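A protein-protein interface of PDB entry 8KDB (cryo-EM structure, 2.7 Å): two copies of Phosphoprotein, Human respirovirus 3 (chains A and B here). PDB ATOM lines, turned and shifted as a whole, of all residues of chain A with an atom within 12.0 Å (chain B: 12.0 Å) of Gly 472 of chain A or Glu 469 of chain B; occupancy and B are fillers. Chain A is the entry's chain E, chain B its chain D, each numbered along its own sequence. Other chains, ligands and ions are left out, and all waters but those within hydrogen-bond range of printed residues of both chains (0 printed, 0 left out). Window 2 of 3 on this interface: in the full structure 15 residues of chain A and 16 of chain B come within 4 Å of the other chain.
O of Gly 472 of chain A lies close to O of Met 467 of chain B, at 3.2 Å.
The side-chain amino group (NZ) of Lys 465 of chain A is in salt-bridge range of the side-chain carboxylate (OE2) of Glu 469 of chain A (2.8 Å).
Lys 465 of chain A touches Leu 464 of chain B (CG to CD2, 3.8 Å). Thr 468 of chain A touches Leu 464 of chain B (CG2 to CD2, 3.98 Å). Lys 465 of chain B touches Thr 468 of chain A. O of Thr 468 of chain A touches N of Met 467 of chain B, at 3.7 Å. Leu 464 of chain B touches Glu 469 of chain A (CD2 to OE2, 3.2 Å). Glu 469 of chain A touches Lys 465 of chain B (CG to O, 3.2 Å). O of Glu 469 of chain A touches CG of Met 467 of chain B (3.1 Å). CG of Glu 469 of chain B touches O of Gly 472 of chain A, 3.3 Å away.
Printed residues of chain B within 4 Å of Lys 465 of chain A: Leu 464. Of the printed residues of chain B, Thr 468 of chain A touches Leu 464, Lys 465 and Met 467. Of the printed residues of chain B, Glu 469 of chain A touches Leu 464 (3.2 Å), Lys 465 (3.2 Å) and Met 467 (3.1 Å). Printed residues of chain A within 4 Å of Leu 464 of chain B: Lys 465, Thr 468 and Glu 469. Of the printed residues of chain A, Lys 465 of chain B touches Thr 468 and Glu 469. Met 467 of chain B touches just these residues of chain A: Thr 468, Glu 469 and Gly 472. No residue of chain A comes within 4 Å of Thr 468 of chain B. Glu 469 of chain B touches just one residue of chain A: Gly 472. The nearest residue of chain A that does not touch Glu 469 of chain B is Gly 471 of chain A (5.7 Å). The nearest printed residue of chain B that does not touch Lys 465 of chain A is Lys 465 of chain B (5.7 Å).
Of the 10 printed residues of chain A, 4 touch a printed residue of chain B. Printed residues of chain A that touch a printed residue of chain B: Lys 465, Thr 468, Glu 469 and Gly 472. Hydrophobic or aromatic side chains of chain B within 4 Å of the printed part of chain A: Leu 464 and Met 467. Along chain B the printed residues that touch a printed residue of chain A span positions 464 to 469. Among the printed residues, no Asp or Glu carboxylate lies within 4 Å of a Lys or Arg side-chain nitrogen of the other chain.
Lys 465 of chain A touches Leu 464 of chain B, but with the chains exchanged Leu 464 of chain A does not touch Lys 465 of chain B (7.3 Å). Thr 468 of chain A touches Met 467 of chain B, but with the chains exchanged Met 467 of chain A does not touch Thr 468 of chain B (9.1 Å). Glu 469 of chain A touches Lys 465 of chain B, but with the chains exchanged Lys 465 of chain A does not touch Glu 469 of chain B (13.4 Å). Gly 472 of chain A touches Met 467 of chain B, but with the chains exchanged Met 467 of chain A does not touch Gly 472 of chain B (18.4 Å). Positions printed for both chains: 464, 465, 466, 467, 468, 469, 470, 471 and 472. Of the 9 pairs that touch across the chains among the printed residues, none has its exchanged pair printed and touching as well.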
ATOM      1  N   ASN A 463       6.703 -22.081  10.564  1.00  0.00           N
ATOM      2  CA  ASN A 463       7.308 -20.752  10.635  1.00  0.00           C
ATOM      3  C   ASN A 463       8.694 -20.813  11.268  1.00  0.00           C
ATOM      4  O   ASN A 463       9.639 -20.175  10.782  1.00  0.00           O
ATOM      5  CB  ASN A 463       6.405 -19.800  11.419  1.00  0.00           C
ATOM      6  CG  ASN A 463       5.174 -19.389  10.641  1.00  0.00           C
ATOM      7  OD1 ASN A 463       4.651 -20.154   9.831  1.00  0.00           O
ATOM      8  ND2 ASN A 463       4.704 -18.172  10.880  1.00  0.00           N
ATOM      9  N   LEU A 464       8.836 -21.585  12.349  1.00  0.00           N
ATOM     10  CA  LEU A 464      10.136 -21.729  12.996  1.00  0.00           C
ATOM     11  C   LEU A 464      11.165 -22.335  12.052  1.00  0.00           C
ATOM     12  O   LEU A 464      12.309 -21.872  11.995  1.00  0.00           O
ATOM     13  CB  LEU A 464       9.999 -22.586  14.255  1.00  0.00           C
ATOM     14  CG  LEU A 464      11.289 -23.000  14.966  1.00  0.00           C
ATOM     15  CD1 LEU A 464      11.894 -21.841  15.735  1.00  0.00           C
ATOM     16  CD2 LEU A 464      11.030 -24.179  15.892  1.00  0.00           C
ATOM     17  N   LYS A 465      10.778 -23.374  11.308  1.00  0.00           N
ATOM     18  CA  LYS A 465      11.709 -24.002  10.375  1.00  0.00           C
ATOM     19  C   LYS A 465      12.139 -23.030   9.284  1.00  0.00           C
ATOM     20  O   LYS A 465      13.328 -22.944   8.951  1.00  0.00           O
ATOM     21  CB  LYS A 465      11.079 -25.248   9.756  1.00  0.00           C
ATOM     22  CG  LYS A 465      11.850 -25.778   8.560  1.00  0.00           C
ATOM     23  CD  LYS A 465      10.993 -26.684   7.699  1.00  0.00           C
ATOM     24  CE  LYS A 465      11.847 -27.596   6.829  1.00  0.00           C
ATOM     25  NZ  LYS A 465      12.379 -28.764   7.584  1.00  0.00           N
ATOM     26  N   ILE A 466      11.187 -22.279   8.725  1.00  0.00           N
ATOM     27  CA  ILE A 466      11.527 -21.328   7.672  1.00  0.00           C
ATOM     28  C   ILE A 466      12.466 -20.257   8.205  1.00  0.00           C
ATOM     29  O   ILE A 466      13.400 -19.830   7.515  1.00  0.00           O
ATOM     30  CB  ILE A 466      10.253 -20.717   7.059  1.00  0.00           C
ATOM     31  CG1 ILE A 466       9.364 -21.816   6.473  1.00  0.00           C
ATOM     32  CG2 ILE A 466      10.609 -19.693   5.990  1.00  0.00           C
ATOM     33  CD1 ILE A 466      10.023 -22.607   5.360  1.00  0.00           C
ATOM     34  N   MET A 467      12.244 -19.808   9.442  1.00  0.00           N
ATOM     35  CA  MET A 467      13.113 -18.773   9.996  1.00  0.00           C
ATOM     36  C   MET A 467      14.502 -19.315  10.324  1.00  0.00           C
ATOM     37  O   MET A 467      15.500 -18.607  10.150  1.00  0.00           O
ATOM     38  CB  MET A 467      12.470 -18.146  11.232  1.00  0.00           C
ATOM     39  CG  MET A 467      11.478 -17.036  10.910  1.00  0.00           C
ATOM     40  SD  MET A 467      10.393 -16.637  12.292  1.00  0.00           S
ATOM     41  CE  MET A 467      11.459 -17.034  13.672  1.00  0.00           C
ATOM     42  N   THR A 468      14.594 -20.560  10.800  1.00  0.00           N
ATOM     43  CA  THR A 468      15.868 -21.070  11.296  1.00  0.00           C
ATOM     44  C   THR A 468      16.755 -21.688  10.222  1.00  0.00           C
ATOM     45  O   THR A 468      17.982 -21.646  10.366  1.00  0.00           O
ATOM     46  CB  THR A 468      15.646 -22.109  12.404  1.00  0.00           C
ATOM     47  OG1 THR A 468      16.906 -22.461  12.986  1.00  0.00           O
ATOM     48  CG2 THR A 468      15.006 -23.370  11.854  1.00  0.00           C
ATOM     49  N   GLU A 469      16.189 -22.264   9.156  1.00  0.00           N
ATOM     50  CA  GLU A 469      17.044 -22.945   8.185  1.00  0.00           C
ATOM     51  C   GLU A 469      17.728 -21.977   7.229  1.00  0.00           C
ATOM     52  O   GLU A 469      18.793 -22.292   6.690  1.00  0.00           O
ATOM     53  CB  GLU A 469      16.256 -23.999   7.405  1.00  0.00           C
ATOM     54  CG  GLU A 469      15.801 -25.178   8.245  1.00  0.00           C
ATOM     55  CD  GLU A 469      15.016 -26.192   7.446  1.00  0.00           C
ATOM     56  OE1 GLU A 469      14.714 -25.917   6.265  1.00  0.00           O
ATOM     57  OE2 GLU A 469      14.719 -27.274   7.991  1.00  0.00           O
ATOM     58  N   ARG A 470      17.136 -20.813   6.982  1.00  0.00           N
ATOM     59  CA  ARG A 470      17.720 -19.834   6.076  1.00  0.00           C
ATOM     60  C   ARG A 470      17.724 -18.472   6.748  1.00  0.00           C
ATOM     61  O   ARG A 470      16.720 -18.065   7.341  1.00  0.00           O
ATOM     62  CB  ARG A 470      16.956 -19.783   4.748  1.00  0.00           C
ATOM     63  CG  ARG A 470      16.905 -21.125   4.028  1.00  0.00           C
ATOM     64  CD  ARG A 470      18.276 -21.519   3.500  1.00  0.00           C
ATOM     65  NE  ARG A 470      18.265 -22.829   2.860  1.00  0.00           N
ATOM     66  CZ  ARG A 470      18.031 -23.035   1.571  1.00  0.00           C
ATOM     67  NH1 ARG A 470      17.788 -22.033   0.743  1.00  0.00           N
ATOM     68  NH2 ARG A 470      18.042 -24.280   1.101  1.00  0.00           N
ATOM     69  N   GLY A 471      18.856 -17.777   6.665  1.00  0.00           N
ATOM     70  CA  GLY A 471      18.984 -16.457   7.239  1.00  0.00           C
ATOM     71  C   GLY A 471      19.169 -16.418   8.739  1.00  0.00           C
ATOM     72  O   GLY A 471      19.169 -15.323   9.315  1.00  0.00           O
ATOM     73  N   GLY A 472      19.330 -17.565   9.390  1.00  0.00           N
ATOM     74  CA  GLY A 472      19.487 -17.607  10.833  1.00  0.00           C
ATOM     75  C   GLY A 472      20.833 -17.100  11.308  1.00  0.00           C
ATOM     76  O   GLY A 472      21.089 -17.019  12.510  1.00  0.00           O
ATOM     77  N   LEU B 464      16.443 -30.689  11.055  1.00  0.00           N
ATOM     78  CA  LEU B 464      16.544 -29.250  10.871  1.00  0.00           C
ATOM     79  C   LEU B 464      17.961 -28.855  10.476  1.00  0.00           C
ATOM     80  O   LEU B 464      18.943 -29.388  10.999  1.00  0.00           O
ATOM     81  CB  LEU B 464      16.153 -28.495  12.143  1.00  0.00           C
ATOM     82  CG  LEU B 464      14.691 -28.094  12.322  1.00  0.00           C
ATOM     83  CD1 LEU B 464      14.502 -27.383  13.651  1.00  0.00           C
ATOM     84  CD2 LEU B 464      14.233 -27.215  11.175  1.00  0.00           C
ATOM     85  N   LYS B 465      18.052 -27.910   9.547  1.00  0.00           N
ATOM     86  CA  LYS B 465      19.305 -27.257   9.198  1.00  0.00           C
ATOM     87  C   LYS B 465      19.418 -25.977  10.014  1.00  0.00           C
ATOM     88  O   LYS B 465      18.461 -25.201  10.082  1.00  0.00           O
ATOM     89  CB  LYS B 465      19.358 -26.935   7.706  1.00  0.00           C
ATOM     90  CG  LYS B 465      19.280 -28.143   6.793  1.00  0.00           C
ATOM     91  CD  LYS B 465      20.524 -29.002   6.887  1.00  0.00           C
ATOM     92  CE  LYS B 465      20.416 -30.206   5.968  1.00  0.00           C
ATOM     93  NZ  LYS B 465      20.442 -29.817   4.533  1.00  0.00           N
ATOM     94  N   ILE B 466      20.569 -25.761  10.640  1.00  0.00           N
ATOM     95  CA  ILE B 466      20.781 -24.596  11.493  1.00  0.00           C
ATOM     96  C   ILE B 466      21.880 -23.736  10.886  1.00  0.00           C
ATOM     97  O   ILE B 466      22.989 -24.221  10.644  1.00  0.00           O
ATOM     98  CB  ILE B 466      21.131 -25.008  12.931  1.00  0.00           C
ATOM     99  CG1 ILE B 466      19.974 -25.789  13.551  1.00  0.00           C
ATOM    100  CG2 ILE B 466      21.450 -23.787  13.773  1.00  0.00           C
ATOM    101  CD1 ILE B 466      20.318 -26.450  14.862  1.00  0.00           C
ATOM    102  N   MET B 467      21.575 -22.465  10.646  1.00  0.00           N
ATOM    103  CA  MET B 467      22.541 -21.512  10.118  1.00  0.00           C
ATOM    104  C   MET B 467      23.024 -20.605  11.242  1.00  0.00           C
ATOM    105  O   MET B 467      22.217 -19.936  11.895  1.00  0.00           O
ATOM    106  CB  MET B 467      21.935 -20.679   8.989  1.00  0.00           C
ATOM    107  CG  MET B 467      21.583 -21.467   7.746  1.00  0.00           C
ATOM    108  SD  MET B 467      23.012 -22.258   6.989  1.00  0.00           S
ATOM    109  CE  MET B 467      23.899 -20.830   6.373  1.00  0.00           C
ATOM    110  N   THR B 468      24.333 -20.585  11.461  1.00  0.00           N
ATOM    111  CA  THR B 468      24.928 -19.667  12.417  1.00  0.00           C
ATOM    112  C   THR B 468      25.055 -18.278  11.803  1.00  0.00           C
ATOM    113  O   THR B 468      25.031 -18.111  10.581  1.00  0.00           O
ATOM    114  CB  THR B 468      26.297 -20.173  12.869  1.00  0.00           C
ATOM    115  OG1 THR B 468      27.168 -20.271  11.737  1.00  0.00           O
ATOM    116  CG2 THR B 468      26.168 -21.543  13.514  1.00  0.00           C
ATOM    117  N   GLU B 469      25.184 -17.274  12.667  1.00  0.00           N
ATOM    118  CA  GLU B 469      25.186 -15.895  12.208  1.00  0.00           C
ATOM    119  C   GLU B 469      26.549 -15.505  11.638  1.00  0.00           C
ATOM    120  O   GLU B 469      27.559 -16.192  11.816  1.00  0.00           O
ATOM    121  CB  GLU B 469      24.801 -14.950  13.345  1.00  0.00           C
ATOM    122  CG  GLU B 469      23.504 -15.316  14.040  1.00  0.00           C
ATOM    123  CD  GLU B 469      22.798 -14.109  14.622  1.00  0.00           C
ATOM    124  OE1 GLU B 469      21.681 -13.791  14.162  1.00  0.00           O
ATOM    125  OE2 GLU B 469      23.364 -13.473  15.536  1.00  0.00           O
ATOM    126  N   ARG B 470      26.558 -14.372  10.941  1.00  0.00           N
ATOM    127  CA  ARG B 470      27.758 -13.814  10.337  1.00  0.00           C
ATOM    128  C   ARG B 470      28.510 -12.971  11.359  1.00  0.00           C
ATOM    129  O   ARG B 470      27.915 -12.125  12.031  1.00  0.00           O
ATOM    130  CB  ARG B 470      27.382 -12.960   9.123  1.00  0.00           C
ATOM    131  CG  ARG B 470      28.545 -12.330   8.374  1.00  0.00           C
ATOM    132  CD  ARG B 470      29.434 -13.348   7.688  1.00  0.00           C
ATOM    133  NE  ARG B 470      30.502 -12.688   6.947  1.00  0.00           N
ATOM    134  CZ  ARG B 470      31.525 -13.313   6.380  1.00  0.00           C
ATOM    135  NH1 ARG B 470      31.644 -14.629   6.425  1.00  0.00           N
ATOM    136  NH2 ARG B 470      32.451 -12.597   5.748  1.00  0.00           N
ATOM    137  N   GLY B 471      29.815 -13.205  11.475  1.00  0.00           N
ATOM    138  CA  GLY B 471      30.652 -12.399  12.332  1.00  0.00           C
ATOM    139  C   GLY B 471      31.147 -11.146  11.636  1.00  0.00           C
ATOM    140  O   GLY B 471      30.981 -10.951  10.433  1.00  0.00           O
ATOM    141  N   GLY B 472      31.771 -10.280  12.420  1.00  0.00           N
ATOM    142  CA  GLY B 472      32.317  -9.035  11.918  1.00  0.00           C
ATOM    143  C   GLY B 472      31.631  -7.830  12.538  1.00  0.00           C
ATOM    144  O   GLY B 472      30.750  -7.942  13.391  1.00  0.00           O
ATOM    145  N   LYS B 473      32.067  -6.659  12.085  1.00  0.00           N
ATOM    146  CA  LYS B 473      31.501  -5.408  12.570  1.00  0.00           C
ATOM    147  C   LYS B 473      30.077  -5.247  12.050  1.00  0.00           C
ATOM    148  O   LYS B 473      29.808  -5.477  10.867  1.00  0.00           O
ATOM    149  CB  LYS B 473      32.372  -4.232  12.132  1.00  0.00           C
ATOM    150  CG  LYS B 473      32.453  -3.107  13.144  1.00  0.00           C
ATOM    151  CD  LYS B 473      33.518  -2.102  12.753  1.00  0.00           C
ATOM    152  CE  LYS B 473      33.325  -0.779  13.470  1.00  0.00           C
ATOM    153  NZ  LYS B 473      33.178  -0.968  14.937  1.00  0.00           N
ATOM    154  N   LYS B 474      29.161  -4.862  12.943  1.00  0.00           N
ATOM    155  CA  LYS B 474      27.750  -4.795  12.576  1.00  0.00           C
ATOM    156  C   LYS B 474      27.492  -3.740  11.508  1.00  0.00           C
ATOM    157  O   LYS B 474      26.753  -3.992  10.549  1.00  0.00           O
ATOM    158  CB  LYS B 474      26.897  -4.519  13.815  1.00  0.00           C
ATOM    159  CG  LYS B 474      26.986  -5.571  14.925  1.00  0.00           C
ATOM    160  CD  LYS B 474      26.311  -6.894  14.559  1.00  0.00           C
ATOM    161  CE  LYS B 474      27.285  -7.904  13.964  1.00  0.00           C
ATOM    162  NZ  LYS B 474      26.642  -9.223  13.712  1.00  0.00           N
